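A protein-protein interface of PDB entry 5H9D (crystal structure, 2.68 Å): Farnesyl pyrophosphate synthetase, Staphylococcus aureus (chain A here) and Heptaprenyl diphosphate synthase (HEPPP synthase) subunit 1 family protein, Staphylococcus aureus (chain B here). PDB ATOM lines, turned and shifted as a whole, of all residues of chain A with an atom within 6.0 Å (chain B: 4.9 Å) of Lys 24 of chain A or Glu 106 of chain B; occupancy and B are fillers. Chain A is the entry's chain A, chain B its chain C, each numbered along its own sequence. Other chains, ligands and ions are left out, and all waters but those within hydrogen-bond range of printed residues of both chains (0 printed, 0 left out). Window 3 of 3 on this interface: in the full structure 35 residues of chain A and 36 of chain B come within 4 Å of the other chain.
OD2 of Asp 25 of chain A is in hydrogen-bond range of OG of Ser 110 of chain B (2.6 Å). NZ of Lys 24 of chain A lies within salt-bridge range of OE2 of Glu 103 of chain B. The backbone NH of Lys 24 of chain A is in hydrogen-bond range of the side-chain carboxylate of Glu 106 of chain B (2.5 Å). The side-chain hydroxyl (OG) of Ser 23 of chain A is in hydrogen-bond range of the side-chain carboxylate (OE2) of Glu 106 of chain B, 2.4 Å away. The backbone carbonyl oxygen (O) of Glu 106 of chain B lies close to the side-chain carboxylate (OD2) of Asp 25 of chain A (3.4 Å). OD1 of Asp 25 of chain A sits at hydrogen-bond distance from OG of Ser 109 of chain B, 2.9 Å away.
The side-chain hydroxyl (OG) of Ser 23 of chain A lies within hydrogen-bond range of the backbone NH (N) of Asp 25 of chain A (2.8 Å). The backbone NH of Leu 28 of chain A lies within hydrogen-bond range of the side-chain carboxylate of Asp 25 of chain A, 3.1 Å away. The backbone NH (N) of Ser 23 of chain A sits at hydrogen-bond distance from the side-chain carboxylate (OE1) of Glu 29 of chain A. The backbone carbonyl oxygen of Glu 106 of chain B is in hydrogen-bond range of the side-chain hydroxyl of Ser 110 of chain B (3.2 Å).
Among the printed residues, merely in contact across the chains: Leu 28 of chain A with Asn 105 of chain B, Leu 28 of chain A with Glu 106 of chain B and Leu 28 of chain A with Ser 109 of chain B.
Printed residues of chain A within 4 Å of Glu 106 of chain B: Ser 23, Lys 24, Asp 25 and Leu 28. Of the printed residues of chain A, Ser 110 of chain B touches Asp 25. Of the printed residues of chain B, Asp 25 of chain A touches Glu 106 (3.4 Å), Ser 109 (2.9 Å) and Ser 110 (2.6 Å). The nearest printed residue of chain B that does not touch Lys 24 of chain A is Ser 110 of chain B (5.1 Å). The nearest printed residue of chain B that does not touch Ser 23 of chain A is Val 102 of chain B (5.9 Å).
Printed residues of chain B that touch a printed residue of chain A: Glu 103, Asn 105, Glu 106, Ser 109 and Ser 110. Of the 8 printed residues of chain A, 4 touch a printed residue of chain B. Among the printed residues, Asp or Glu carboxylates within 4 Å of a Lys or Arg side-chain nitrogen of the other chain: Lys 24 of chain A with Glu 103 of chain B (3.7 Å).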
ATOM      1  N   LYS A  22     -12.341  -6.102  26.561  1.00  0.00           N
ATOM      2  CA  LYS A  22     -12.715  -5.188  25.501  1.00  0.00           C
ATOM      3  C   LYS A  22     -12.190  -5.704  24.162  1.00  0.00           C
ATOM      4  O   LYS A  22     -11.054  -6.188  24.068  1.00  0.00           O
ATOM      5  CB  LYS A  22     -12.206  -3.787  25.858  1.00  0.00           C
ATOM      6  CG  LYS A  22     -12.933  -3.280  27.099  1.00  0.00           C
ATOM      7  CD  LYS A  22     -12.635  -1.848  27.469  1.00  0.00           C
ATOM      8  CE  LYS A  22     -13.612  -1.389  28.567  1.00  0.00           C
ATOM      9  NZ  LYS A  22     -13.323   0.000  29.061  1.00  0.00           N
ATOM     10  N   SER A  23     -13.019  -5.629  23.127  1.00  0.00           N
ATOM     11  CA  SER A  23     -12.598  -6.133  21.832  1.00  0.00           C
ATOM     12  C   SER A  23     -12.938  -5.266  20.624  1.00  0.00           C
ATOM     13  O   SER A  23     -13.849  -4.454  20.655  1.00  0.00           O
ATOM     14  CB  SER A  23     -13.190  -7.551  21.643  1.00  0.00           C
ATOM     15  OG  SER A  23     -13.255  -7.977  20.291  1.00  0.00           O
ATOM     16  N   LYS A  24     -12.188  -5.473  19.546  1.00  0.00           N
ATOM     17  CA  LYS A  24     -12.432  -4.785  18.312  1.00  0.00           C
ATOM     18  C   LYS A  24     -13.791  -5.266  17.796  1.00  0.00           C
ATOM     19  O   LYS A  24     -14.442  -4.563  17.025  1.00  0.00           O
ATOM     20  CB  LYS A  24     -11.338  -5.106  17.315  1.00  0.00           C
ATOM     21  CG  LYS A  24     -10.080  -4.295  17.523  1.00  0.00           C
ATOM     22  CD  LYS A  24      -9.224  -4.232  16.261  1.00  0.00           C
ATOM     23  CE  LYS A  24      -7.781  -4.757  16.509  1.00  0.00           C
ATOM     24  NZ  LYS A  24      -7.016  -5.041  15.218  1.00  0.00           N
ATOM     25  N   ASP A  25     -14.215  -6.471  18.193  1.00  0.00           N
ATOM     26  CA  ASP A  25     -15.536  -6.985  17.790  1.00  0.00           C
ATOM     27  C   ASP A  25     -16.481  -6.805  18.966  1.00  0.00           C
ATOM     28  O   ASP A  25     -16.261  -7.333  20.057  1.00  0.00           O
ATOM     29  CB  ASP A  25     -15.524  -8.478  17.377  1.00  0.00           C
ATOM     30  CG  ASP A  25     -16.938  -8.997  16.989  1.00  0.00           C
ATOM     31  OD1 ASP A  25     -17.758  -9.314  17.888  1.00  0.00           O
ATOM     32  OD2 ASP A  25     -17.243  -9.085  15.776  1.00  0.00           O
ATOM     33  N   SER A  26     -17.543  -6.066  18.690  1.00  0.00           N
ATOM     34  CA  SER A  26     -18.568  -5.698  19.638  1.00  0.00           C
ATOM     35  C   SER A  26     -19.257  -6.850  20.391  1.00  0.00           C
ATOM     36  O   SER A  26     -19.335  -6.851  21.617  1.00  0.00           O
ATOM     37  CB  SER A  26     -19.573  -4.837  18.884  1.00  0.00           C
ATOM     38  OG  SER A  26     -20.679  -4.498  19.685  1.00  0.00           O
ATOM     39  N   LEU A  28     -18.305 -10.040  20.866  1.00  0.00           N
ATOM     40  CA  LEU A  28     -17.388 -10.739  21.753  1.00  0.00           C
ATOM     41  C   LEU A  28     -17.230  -9.947  23.035  1.00  0.00           C
ATOM     42  O   LEU A  28     -17.051 -10.543  24.085  1.00  0.00           O
ATOM     43  CB  LEU A  28     -16.019 -10.930  21.104  1.00  0.00           C
ATOM     44  CG  LEU A  28     -15.651 -12.308  20.553  1.00  0.00           C
ATOM     45  CD1 LEU A  28     -16.909 -13.095  20.182  1.00  0.00           C
ATOM     46  CD2 LEU A  28     -14.744 -12.134  19.365  1.00  0.00           C
ATOM     47  N   GLU A  29     -17.308  -8.613  22.954  1.00  0.00           N
ATOM     48  CA  GLU A  29     -17.183  -7.768  24.136  1.00  0.00           C
ATOM     49  C   GLU A  29     -18.410  -7.840  25.047  1.00  0.00           C
ATOM     50  O   GLU A  29     -18.282  -7.903  26.275  1.00  0.00           O
ATOM     51  CB  GLU A  29     -16.954  -6.318  23.740  1.00  0.00           C
ATOM     52  CG  GLU A  29     -16.596  -5.453  24.911  1.00  0.00           C
ATOM     53  CD  GLU A  29     -15.977  -4.165  24.475  1.00  0.00           C
ATOM     54  OE1 GLU A  29     -15.204  -4.212  23.491  1.00  0.00           O
ATOM     55  OE2 GLU A  29     -16.254  -3.118  25.122  1.00  0.00           O
ATOM     56  N   PHE A 112     -11.765 -16.619  22.098  1.00  0.00           N
ATOM     57  CA  PHE A 112     -11.345 -15.270  22.442  1.00  0.00           C
ATOM     58  C   PHE A 112     -10.778 -15.234  23.870  1.00  0.00           C
ATOM     59  O   PHE A 112      -9.642 -14.834  24.085  1.00  0.00           O
ATOM     60  CB  PHE A 112     -12.574 -14.357  22.275  1.00  0.00           C
ATOM     61  CG  PHE A 112     -12.386 -12.942  22.729  1.00  0.00           C
ATOM     62  CD1 PHE A 112     -11.585 -12.066  22.016  1.00  0.00           C
ATOM     63  CD2 PHE A 112     -13.063 -12.466  23.858  1.00  0.00           C
ATOM     64  CE1 PHE A 112     -11.462 -10.732  22.412  1.00  0.00           C
ATOM     65  CE2 PHE A 112     -12.944 -11.145  24.256  1.00  0.00           C
ATOM     66  CZ  PHE A 112     -12.142 -10.275  23.531  1.00  0.00           C
ATOM     67  N   VAL B 102      -6.622 -13.861  18.976  1.00  0.00           N
ATOM     68  CA  VAL B 102      -7.825 -13.111  19.350  1.00  0.00           C
ATOM     69  C   VAL B 102      -8.357 -12.338  18.151  1.00  0.00           C
ATOM     70  O   VAL B 102      -9.556 -12.231  17.978  1.00  0.00           O
ATOM     71  CB  VAL B 102      -7.643 -12.130  20.627  1.00  0.00           C
ATOM     72  CG1 VAL B 102      -6.277 -12.257  21.242  1.00  0.00           C
ATOM     73  CG2 VAL B 102      -7.971 -10.699  20.266  1.00  0.00           C
ATOM     74  N   GLU B 103      -7.472 -11.841  17.302  1.00  0.00           N
ATOM     75  CA  GLU B 103      -7.903 -11.091  16.123  1.00  0.00           C
ATOM     76  C   GLU B 103      -8.676 -11.940  15.111  1.00  0.00           C
ATOM     77  O   GLU B 103      -9.742 -11.551  14.600  1.00  0.00           O
ATOM     78  CB  GLU B 103      -6.697 -10.455  15.450  1.00  0.00           C
ATOM     79  CG  GLU B 103      -7.033  -9.836  14.120  1.00  0.00           C
ATOM     80  CD  GLU B 103      -5.974  -8.881  13.636  1.00  0.00           C
ATOM     81  OE1 GLU B 103      -4.779  -9.140  13.920  1.00  0.00           O
ATOM     82  OE2 GLU B 103      -6.342  -7.884  12.966  1.00  0.00           O
ATOM     83  N   ILE B 104      -8.109 -13.103  14.801  1.00  0.00           N
ATOM     84  CA  ILE B 104      -8.769 -14.030  13.889  1.00  0.00           C
ATOM     85  C   ILE B 104     -10.186 -14.245  14.401  1.00  0.00           C
ATOM     86  O   ILE B 104     -11.145 -14.117  13.631  1.00  0.00           O
ATOM     87  CB  ILE B 104      -8.040 -15.375  13.851  1.00  0.00           C
ATOM     88  CG1 ILE B 104      -6.706 -15.218  13.107  1.00  0.00           C
ATOM     89  CG2 ILE B 104      -8.915 -16.425  13.212  1.00  0.00           C
ATOM     90  CD1 ILE B 104      -6.810 -14.476  11.750  1.00  0.00           C
ATOM     91  N   ASN B 105     -10.309 -14.551  15.701  1.00  0.00           N
ATOM     92  CA  ASN B 105     -11.609 -14.775  16.343  1.00  0.00           C
ATOM     93  C   ASN B 105     -12.525 -13.568  16.315  1.00  0.00           C
ATOM     94  O   ASN B 105     -13.713 -13.710  16.116  1.00  0.00           O
ATOM     95  CB  ASN B 105     -11.400 -15.256  17.772  1.00  0.00           C
ATOM     96  CG  ASN B 105     -10.909 -16.670  17.812  1.00  0.00           C
ATOM     97  OD1 ASN B 105     -11.597 -17.602  17.406  1.00  0.00           O
ATOM     98  ND2 ASN B 105      -9.700 -16.841  18.277  1.00  0.00           N
ATOM     99  N   GLU B 106     -11.963 -12.382  16.510  1.00  0.00           N
ATOM    100  CA  GLU B 106     -12.746 -11.143  16.433  1.00  0.00           C
ATOM    101  C   GLU B 106     -13.244 -10.976  14.975  1.00  0.00           C
ATOM    102  O   GLU B 106     -14.423 -10.674  14.749  1.00  0.00           O
ATOM    103  CB  GLU B 106     -11.901  -9.903  16.833  1.00  0.00           C
ATOM    104  CG  GLU B 106     -11.725  -9.669  18.311  1.00  0.00           C
ATOM    105  CD  GLU B 106     -10.735  -8.515  18.615  1.00  0.00           C
ATOM    106  OE1 GLU B 106      -9.679  -8.437  17.943  1.00  0.00           O
ATOM    107  OE2 GLU B 106     -10.985  -7.691  19.529  1.00  0.00           O
ATOM    108  N   LEU B 107     -12.360 -11.168  13.991  1.00  0.00           N
ATOM    109  CA  LEU B 107     -12.796 -11.017  12.613  1.00  0.00           C
ATOM    110  C   LEU B 107     -13.901 -12.004  12.257  1.00  0.00           C
ATOM    111  O   LEU B 107     -14.898 -11.596  11.683  1.00  0.00           O
ATOM    112  CB  LEU B 107     -11.625 -11.145  11.641  1.00  0.00           C
ATOM    113  CG  LEU B 107     -10.571 -10.035  11.767  1.00  0.00           C
ATOM    114  CD1 LEU B 107      -9.299 -10.416  11.015  1.00  0.00           C
ATOM    115  CD2 LEU B 107     -11.125  -8.752  11.262  1.00  0.00           C
ATOM    116  N   LYS B 108     -13.752 -13.290  12.595  1.00  0.00           N
ATOM    117  CA  LYS B 108     -14.818 -14.262  12.292  1.00  0.00           C
ATOM    118  C   LYS B 108     -16.136 -13.828  12.949  1.00  0.00           C
ATOM    119  O   LYS B 108     -17.195 -13.906  12.325  1.00  0.00           O
ATOM    120  CB  LYS B 108     -14.448 -15.675  12.751  1.00  0.00           C
ATOM    121  CG  LYS B 108     -13.463 -16.401  11.850  1.00  0.00           C
ATOM    122  CD  LYS B 108     -12.958 -17.717  12.428  1.00  0.00           C
ATOM    123  CE  LYS B 108     -11.883 -18.321  11.511  1.00  0.00           C
ATOM    124  NZ  LYS B 108     -11.146 -19.540  12.051  1.00  0.00           N
ATOM    125  N   SER B 109     -16.080 -13.360  14.190  1.00  0.00           N
ATOM    126  CA  SER B 109     -17.295 -12.901  14.863  1.00  0.00           C
ATOM    127  C   SER B 109     -17.938 -11.759  14.069  1.00  0.00           C
ATOM    128  O   SER B 109     -19.165 -11.714  13.878  1.00  0.00           O
ATOM    129  CB  SER B 109     -16.982 -12.412  16.271  1.00  0.00           C
ATOM    130  OG  SER B 109     -18.159 -11.974  16.914  1.00  0.00           O
ATOM    131  N   SER B 110     -17.098 -10.835  13.623  1.00  0.00           N
ATOM    132  CA  SER B 110     -17.562  -9.718  12.851  1.00  0.00           C
ATOM    133  C   SER B 110     -18.227 -10.189  11.547  1.00  0.00           C
ATOM    134  O   SER B 110     -19.250  -9.639  11.131  1.00  0.00           O
ATOM    135  CB  SER B 110     -16.383  -8.780  12.563  1.00  0.00           C
ATOM    136  OG  SER B 110     -15.985  -8.067  13.721  1.00  0.00           O
